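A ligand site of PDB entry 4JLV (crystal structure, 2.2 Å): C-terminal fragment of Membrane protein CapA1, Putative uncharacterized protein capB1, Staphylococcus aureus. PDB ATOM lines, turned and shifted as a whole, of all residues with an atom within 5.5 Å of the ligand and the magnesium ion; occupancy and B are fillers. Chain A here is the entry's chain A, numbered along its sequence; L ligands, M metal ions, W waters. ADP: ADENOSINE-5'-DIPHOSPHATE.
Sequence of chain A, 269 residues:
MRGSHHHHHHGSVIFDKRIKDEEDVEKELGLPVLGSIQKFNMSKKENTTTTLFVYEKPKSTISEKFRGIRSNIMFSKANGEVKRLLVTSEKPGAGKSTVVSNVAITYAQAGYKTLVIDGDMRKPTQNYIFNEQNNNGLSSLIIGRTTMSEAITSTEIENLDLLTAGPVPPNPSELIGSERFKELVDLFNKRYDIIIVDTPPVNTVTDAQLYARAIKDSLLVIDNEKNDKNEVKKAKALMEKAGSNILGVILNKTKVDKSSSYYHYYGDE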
ATOM      1  N   ILE A  37      12.928  37.263 -13.505  1.00  0.00           N
ATOM      2  CA  ILE A  37      14.145  36.579 -13.912  1.00  0.00           C
ATOM      3  C   ILE A  37      14.428  36.914 -15.371  1.00  0.00           C
ATOM      4  O   ILE A  37      13.573  36.718 -16.237  1.00  0.00           O
ATOM      5  CB  ILE A  37      14.020  35.033 -13.812  1.00  0.00           C
ATOM      6  CG1 ILE A  37      13.621  34.602 -12.390  1.00  0.00           C
ATOM      7  CG2 ILE A  37      15.306  34.380 -14.245  1.00  0.00           C
ATOM      8  CD1 ILE A  37      14.472  35.215 -11.276  1.00  0.00           C
ATOM      9  N   GLN A  38      15.627  37.404 -15.648  1.00  0.00           N
ATOM     10  CA  GLN A  38      15.977  37.780 -17.016  1.00  0.00           C
ATOM     11  C   GLN A  38      16.246  36.538 -17.872  1.00  0.00           C
ATOM     12  O   GLN A  38      16.532  35.466 -17.343  1.00  0.00           O
ATOM     13  CB  GLN A  38      17.197  38.710 -17.027  1.00  0.00           C
ATOM     14  CG  GLN A  38      18.541  38.005 -16.785  1.00  0.00           C
ATOM     15  CD  GLN A  38      19.042  38.150 -15.352  1.00  0.00           C
ATOM     16  OE1 GLN A  38      18.316  37.882 -14.398  1.00  0.00           O
ATOM     17  NE2 GLN A  38      20.293  38.606 -15.204  1.00  0.00           N
ATOM     18  N   LYS A  39      16.162  36.701 -19.192  1.00  0.00           N
ATOM     19  CA  LYS A  39      16.461  35.615 -20.134  1.00  0.00           C
ATOM     20  C   LYS A  39      17.969  35.387 -20.212  1.00  0.00           C
ATOM     21  O   LYS A  39      18.741  36.233 -19.760  1.00  0.00           O
ATOM     22  CB  LYS A  39      15.883  35.927 -21.516  1.00  0.00           C
ATOM     23  CG  LYS A  39      15.497  34.697 -22.338  1.00  0.00           C
ATOM     24  CD  LYS A  39      15.265  35.046 -23.805  1.00  0.00           C
ATOM     25  CE  LYS A  39      14.730  33.869 -24.611  1.00  0.00           C
ATOM     26  NZ  LYS A  39      13.280  33.609 -24.347  1.00  0.00           N
ATOM     27  N   PHE A  40      18.410  34.254 -20.770  1.00  0.00           N
ATOM     28  CA  PHE A  40      19.847  33.993 -20.899  1.00  0.00           C
ATOM     29  C   PHE A  40      20.187  32.980 -22.002  1.00  0.00           C
ATOM     30  O   PHE A  40      21.294  32.421 -22.021  1.00  0.00           O
ATOM     31  CB  PHE A  40      20.446  33.554 -19.563  1.00  0.00           C
ATOM     32  CG  PHE A  40      19.687  32.449 -18.874  1.00  0.00           C
ATOM     33  CD1 PHE A  40      19.697  31.163 -19.369  1.00  0.00           C
ATOM     34  CD2 PHE A  40      18.956  32.703 -17.723  1.00  0.00           C
ATOM     35  CE1 PHE A  40      18.998  30.138 -18.748  1.00  0.00           C
ATOM     36  CE2 PHE A  40      18.246  31.694 -17.082  1.00  0.00           C
ATOM     37  CZ  PHE A  40      18.264  30.413 -17.597  1.00  0.00           C
ATOM     38  N   ILE A  62      21.470  37.099 -11.540  1.00  0.00           N
ATOM     39  CA  ILE A  62      20.276  36.252 -11.558  1.00  0.00           C
ATOM     40  C   ILE A  62      20.077  35.516 -10.219  1.00  0.00           C
ATOM     41  O   ILE A  62      18.947  35.297  -9.775  1.00  0.00           O
ATOM     42  CB  ILE A  62      20.291  35.286 -12.757  1.00  0.00           C
ATOM     43  CG1 ILE A  62      18.976  34.506 -12.844  1.00  0.00           C
ATOM     44  CG2 ILE A  62      21.485  34.346 -12.686  1.00  0.00           C
ATOM     45  CD1 ILE A  62      18.836  33.705 -14.099  1.00  0.00           C
ATOM     46  N   SER A  89       2.212  27.355 -13.603  1.00  0.00           N
ATOM     47  CA  SER A  89       2.137  28.300 -14.707  1.00  0.00           C
ATOM     48  C   SER A  89       0.922  27.958 -15.566  1.00  0.00           C
ATOM     49  O   SER A  89       0.310  26.900 -15.398  1.00  0.00           O
ATOM     50  CB  SER A  89       3.383  28.169 -15.576  1.00  0.00           C
ATOM     51  OG  SER A  89       3.335  26.930 -16.296  1.00  0.00           O
ATOM     52  N   LYS A  91       0.956  27.690 -19.009  1.00  0.00           N
ATOM     53  CA  LYS A  91       1.331  26.911 -20.177  1.00  0.00           C
ATOM     54  C   LYS A  91       2.724  26.306 -19.996  1.00  0.00           C
ATOM     55  O   LYS A  91       3.519  26.815 -19.192  1.00  0.00           O
ATOM     56  CB  LYS A  91       1.384  27.829 -21.386  1.00  0.00           C
ATOM     57  CG  LYS A  91       2.555  28.789 -21.312  1.00  0.00           C
ATOM     58  CD  LYS A  91       2.720  29.609 -22.569  1.00  0.00           C
ATOM     59  CE  LYS A  91       3.850  30.611 -22.414  1.00  0.00           C
ATOM     60  NZ  LYS A  91       5.183  30.003 -22.107  1.00  0.00           N
ATOM     61  N   PRO A  92       3.037  25.219 -20.735  1.00  0.00           N
ATOM     62  CA  PRO A  92       4.385  24.631 -20.699  1.00  0.00           C
ATOM     63  C   PRO A  92       5.506  25.631 -21.003  1.00  0.00           C
ATOM     64  O   PRO A  92       5.271  26.610 -21.715  1.00  0.00           O
ATOM     65  CB  PRO A  92       4.334  23.544 -21.800  1.00  0.00           C
ATOM     66  CG  PRO A  92       2.896  23.170 -21.908  1.00  0.00           C
ATOM     67  CD  PRO A  92       2.095  24.418 -21.558  1.00  0.00           C
ATOM     68  N   GLY A  93       6.696  25.385 -20.471  1.00  0.00           N
ATOM     69  CA  GLY A  93       7.872  26.154 -20.820  1.00  0.00           C
ATOM     70  C   GLY A  93       8.049  27.486 -20.093  1.00  0.00           C
ATOM     71  O   GLY A  93       9.033  28.194 -20.334  1.00  0.00           O
ATOM     72  N   ALA A  94       7.109  27.831 -19.215  1.00  0.00           N
ATOM     73  CA  ALA A  94       7.157  29.115 -18.502  1.00  0.00           C
ATOM     74  C   ALA A  94       8.409  29.292 -17.650  1.00  0.00           C
ATOM     75  O   ALA A  94       8.891  30.403 -17.462  1.00  0.00           O
ATOM     76  CB  ALA A  94       5.923  29.280 -17.643  1.00  0.00           C
ATOM     77  N   GLY A  95       8.934  28.191 -17.125  1.00  0.00           N
ATOM     78  CA  GLY A  95      10.113  28.260 -16.269  1.00  0.00           C
ATOM     79  C   GLY A  95       9.810  27.841 -14.833  1.00  0.00           C
ATOM     80  O   GLY A  95      10.560  28.177 -13.919  1.00  0.00           O
ATOM     81  N   LYS A  96       8.698  27.113 -14.655  1.00  0.00           N
ATOM     82  CA  LYS A  96       8.334  26.523 -13.373  1.00  0.00           C
ATOM     83  C   LYS A  96       9.521  25.830 -12.739  1.00  0.00           C
ATOM     84  O   LYS A  96       9.932  26.152 -11.628  1.00  0.00           O
ATOM     85  CB  LYS A  96       7.231  25.471 -13.553  1.00  0.00           C
ATOM     86  CG  LYS A  96       5.826  25.991 -13.675  1.00  0.00           C
ATOM     87  CD  LYS A  96       4.858  24.855 -13.921  1.00  0.00           C
ATOM     88  CE  LYS A  96       5.254  24.044 -15.160  1.00  0.00           C
ATOM     89  NZ  LYS A  96       5.123  24.886 -16.400  1.00  0.00           N
ATOM     90  N   SER A  97      10.045  24.850 -13.457  1.00  0.00           N
ATOM     91  CA  SER A  97      11.074  23.998 -12.930  1.00  0.00           C
ATOM     92  C   SER A  97      12.334  24.777 -12.551  1.00  0.00           C
ATOM     93  O   SER A  97      12.926  24.532 -11.506  1.00  0.00           O
ATOM     94  CB  SER A  97      11.388  22.888 -13.933  1.00  0.00           C
ATOM     95  OG  SER A  97      10.270  21.996 -14.041  1.00  0.00           O
ATOM     96  N   THR A  98      12.717  25.748 -13.380  1.00  0.00           N
ATOM     97  CA  THR A  98      13.894  26.566 -13.095  1.00  0.00           C
ATOM     98  C   THR A  98      13.669  27.368 -11.824  1.00  0.00           C
ATOM     99  O   THR A  98      14.580  27.520 -11.011  1.00  0.00           O
ATOM    100  CB  THR A  98      14.210  27.509 -14.258  1.00  0.00           C
ATOM    101  OG1 THR A  98      14.366  26.757 -15.459  1.00  0.00           O
ATOM    102  CG2 THR A  98      15.501  28.277 -13.981  1.00  0.00           C
ATOM    103  N   VAL A  99      12.443  27.868 -11.649  1.00  0.00           N
ATOM    104  CA  VAL A  99      12.085  28.609 -10.441  1.00  0.00           C
ATOM    105  C   VAL A  99      12.117  27.687  -9.232  1.00  0.00           C
ATOM    106  O   VAL A  99      12.713  28.023  -8.217  1.00  0.00           O
ATOM    107  CB  VAL A  99      10.682  29.280 -10.592  1.00  0.00           C
ATOM    108  CG1 VAL A  99      10.170  29.793  -9.252  1.00  0.00           C
ATOM    109  CG2 VAL A  99      10.747  30.414 -11.602  1.00  0.00           C
ATOM    110  N   ASP A 120       5.610  16.996 -11.060  1.00  0.00           N
ATOM    111  CA  ASP A 120       5.259  16.803 -12.462  1.00  0.00           C
ATOM    112  C   ASP A 120       5.554  15.344 -12.855  1.00  0.00           C
ATOM    113  O   ASP A 120       6.688  14.986 -13.229  1.00  0.00           O
ATOM    114  CB  ASP A 120       5.992  17.788 -13.374  1.00  0.00           C
ATOM    115  CG  ASP A 120       5.423  17.799 -14.790  1.00  0.00           C
ATOM    116  OD1 ASP A 120       4.902  16.767 -15.235  1.00  0.00           O
ATOM    117  OD2 ASP A 120       5.494  18.851 -15.461  1.00  0.00           O
ATOM    118  N   LYS A 123       5.828  15.078 -17.239  1.00  0.00           N
ATOM    119  CA  LYS A 123       7.157  15.314 -17.793  1.00  0.00           C
ATOM    120  C   LYS A 123       8.134  15.735 -16.715  1.00  0.00           C
ATOM    121  O   LYS A 123       8.546  16.887 -16.665  1.00  0.00           O
ATOM    122  CB  LYS A 123       7.109  16.345 -18.940  1.00  0.00           C
ATOM    123  CG  LYS A 123       6.334  15.828 -20.175  1.00  0.00           C
ATOM    124  CD  LYS A 123       6.240  16.848 -21.328  1.00  0.00           C
ATOM    125  CE  LYS A 123       7.524  16.909 -22.179  1.00  0.00           C
ATOM    126  NZ  LYS A 123       7.941  15.587 -22.768  1.00  0.00           N
ATOM    127  N   THR A 125      11.282  16.635 -14.445  1.00  0.00           N
ATOM    128  CA  THR A 125      12.474  17.340 -14.892  1.00  0.00           C
ATOM    129  C   THR A 125      13.473  17.669 -13.780  1.00  0.00           C
ATOM    130  O   THR A 125      14.651  17.889 -14.072  1.00  0.00           O
ATOM    131  CB  THR A 125      12.096  18.583 -15.730  1.00  0.00           C
ATOM    132  OG1 THR A 125      13.210  18.964 -16.552  1.00  0.00           O
ATOM    133  CG2 THR A 125      11.778  19.695 -14.876  1.00  0.00           C
ATOM    134  N   ASP A 198       7.172  21.262  -7.616  1.00  0.00           N
ATOM    135  CA  ASP A 198       7.045  21.537  -9.046  1.00  0.00           C
ATOM    136  C   ASP A 198       5.764  20.833  -9.533  1.00  0.00           C
ATOM    137  O   ASP A 198       5.348  19.833  -8.934  1.00  0.00           O
ATOM    138  CB  ASP A 198       8.265  20.982  -9.775  1.00  0.00           C
ATOM    139  CG  ASP A 198       8.476  21.616 -11.136  1.00  0.00           C
ATOM    140  OD1 ASP A 198       7.645  22.432 -11.537  1.00  0.00           O
ATOM    141  OD2 ASP A 198       9.480  21.268 -11.802  1.00  0.00           O
ATOM    142  N   ASN A 252       9.115  35.714 -15.874  1.00  0.00           N
ATOM    143  CA  ASN A 252      10.308  35.014 -16.311  1.00  0.00           C
ATOM    144  C   ASN A 252      10.690  35.423 -17.726  1.00  0.00           C
ATOM    145  O   ASN A 252       9.827  35.841 -18.497  1.00  0.00           O
ATOM    146  CB  ASN A 252      10.072  33.499 -16.247  1.00  0.00           C
ATOM    147  CG  ASN A 252      11.334  32.698 -16.501  1.00  0.00           C
ATOM    148  OD1 ASN A 252      12.406  33.032 -15.994  1.00  0.00           O
ATOM    149  ND2 ASN A 252      11.219  31.636 -17.286  1.00  0.00           N
ATOM    150  N   LYS A 253      11.975  35.290 -18.076  1.00  0.00           N
ATOM    151  CA  LYS A 253      12.491  35.584 -19.417  1.00  0.00           C
ATOM    152  C   LYS A 253      12.292  37.050 -19.824  1.00  0.00           C
ATOM    153  O   LYS A 253      12.159  37.365 -21.006  1.00  0.00           O
ATOM    154  CB  LYS A 253      11.844  34.660 -20.480  1.00  0.00           C
ATOM    155  CG  LYS A 253      11.973  33.184 -20.161  1.00  0.00           C
ATOM    156  CD  LYS A 253      11.018  32.350 -21.004  1.00  0.00           C
ATOM    157  CE  LYS A 253      11.095  30.882 -20.593  1.00  0.00           C
ATOM    158  NZ  LYS A 253      10.703  29.951 -21.698  1.00  0.00           N
HETATM  159  PB  ADP L   1       8.470  24.507 -17.303  1.00  0.00           P
HETATM  160  O1B ADP L   1       7.809  23.576 -18.339  1.00  0.00           O
HETATM  161  O2B ADP L   1       8.891  23.808 -16.027  1.00  0.00           O
HETATM  162  O3B ADP L   1       7.708  25.805 -17.077  1.00  0.00           O
HETATM  163  PA  ADP L   1      11.346  24.991 -17.543  1.00  0.00           P
HETATM  164  O1A ADP L   1      11.916  23.597 -17.711  1.00  0.00           O
HETATM  165  O2A ADP L   1      11.518  25.705 -16.213  1.00  0.00           O
HETATM  166  O3A ADP L   1       9.813  24.971 -18.074  1.00  0.00           O
HETATM  167  O5' ADP L   1      12.000  25.931 -18.678  1.00  0.00           O
HETATM  168  C5' ADP L   1      11.841  25.588 -20.054  1.00  0.00           C
HETATM  169  C4' ADP L   1      13.136  25.961 -20.792  1.00  0.00           C
HETATM  170  O4' ADP L   1      13.292  27.391 -20.707  1.00  0.00           O
HETATM  171  C3' ADP L   1      14.365  25.308 -20.165  1.00  0.00           C
HETATM  172  O3' ADP L   1      15.169  24.724 -21.185  1.00  0.00           O
HETATM  173  C2' ADP L   1      15.105  26.449 -19.472  1.00  0.00           C
HETATM  174  O2' ADP L   1      16.531  26.334 -19.556  1.00  0.00           O
HETATM  175  C1' ADP L   1      14.585  27.707 -20.165  1.00  0.00           C
HETATM  176  N9  ADP L   1      14.469  28.869 -19.250  1.00  0.00           N
HETATM  177  C8  ADP L   1      13.765  28.923 -18.096  1.00  0.00           C
HETATM  178  N7  ADP L   1      13.889  30.131 -17.506  1.00  0.00           N
HETATM  179  C5  ADP L   1      14.690  30.885 -18.290  1.00  0.00           C
HETATM  180  C6  ADP L   1      15.237  32.259 -18.262  1.00  0.00           C
HETATM  181  N6  ADP L   1      14.934  33.117 -17.252  1.00  0.00           N
HETATM  182  N1  ADP L   1      16.035  32.636 -19.281  1.00  0.00           N
HETATM  183  C2  ADP L   1      16.344  31.811 -20.294  1.00  0.00           C
HETATM  184  N3  ADP L   1      15.892  30.554 -20.391  1.00  0.00           N
HETATM  185  C4  ADP L   1      15.070  30.043 -19.436  1.00  0.00           C
HETATM  186 MG    MG M   1       9.156  21.463 -16.342  1.00  0.00          MG
HETATM  187  O   HOH W   1       7.667  22.124 -14.302  1.00  0.00           O
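CG2 of Thr 125 touches the magnesium ion (3.5 Å).
Of the 21 residues printed, 2 come within 4 Å of the magnesium ion.
The nearest printed residue that does not touch the magnesium ion is Asp 198 (4.6 Å).
Merely in contact with the ligand: Ile 37, Lys 39 and Lys 253.
Within 4 Å of the ligand: Ile 37, Gln 38, Lys 39, Phe 40, Gly 93, Ala 94, Gly 95, Lys 96, Ser 97, Thr 98, Asn 252 and Lys 253.
Water W1 lies within hydrogen-bond range of the side-chain hydroxyl (OG) of Ser 97 (2.6 Å) and the side-chain carboxylate (OD1) of Asp 198 (2.8 Å).
The magnesium ion is bound by an oxygen (O2B) of the ligand (2.4 Å).
The magnesium ion has one donor atom within binding distance.
Slightly farther from the magnesium ion lies water W1 (2.6 Å).
Slightly farther from the magnesium ion lies OG of Ser 97 (2.6 Å).
The backbone carbonyl oxygen (O) of Gln 38 is in hydrogen-bond range of a nitrogen (N6) of the ligand, 2.8 Å away.
The backbone NH (N) of Thr 98 lies within hydrogen-bond range of an oxygen (O2A) of the ligand, 3.1 Å away.
N of Ala 94 lies within hydrogen-bond range of O3B of the ligand (3.0 Å).
N of Lys 96 lies within hydrogen-bond range of O3B of the ligand (2.9 Å).
An oxygen (O2A) of the ligand lies within hydrogen-bond range of the backbone NH (N) of Ser 97 (3.2 Å).
N of Phe 40 sits close to N1 of the ligand (3.2 Å).
OD1 of Asn 252 sits at hydrogen-bond distance from N6 of the ligand (2.8 Å).
The side-chain hydroxyl (OG1) of Thr 98 lies within hydrogen-bond range of an oxygen (O2A) of the ligand (3.1 Å).
N of Gly 95 lies within hydrogen-bond range of O3B of the ligand (2.7 Å).
NZ of Lys 96 lies within salt-bridge range of O3B of the ligand.
N of Gly 93 sits at hydrogen-bond distance from O1B of the ligand.
An oxygen (O2B) of the ligand sits close to the side-chain hydroxyl (OG) of Ser 97, 3.0 Å away.
The side-chain amide nitrogen (ND2) of Asn 252 sits at hydrogen-bond distance from the backbone carbonyl oxygen (O) of Ala 94 (2.6 Å).
O of Gly 93 lies within hydrogen-bond range of NZ of Lys 253, 2.8 Å away.
The side-chain hydroxyl (OG) of Ser 97 is in hydrogen-bond range of the side-chain carboxylate (OD2) of Asp 198 (2.5 Å).
OG of Ser 89 sits at hydrogen-bond distance from NZ of Lys 96 (2.7 Å).
O of Ile 37 lies within hydrogen-bond range of N of Lys 253 (2.8 Å).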
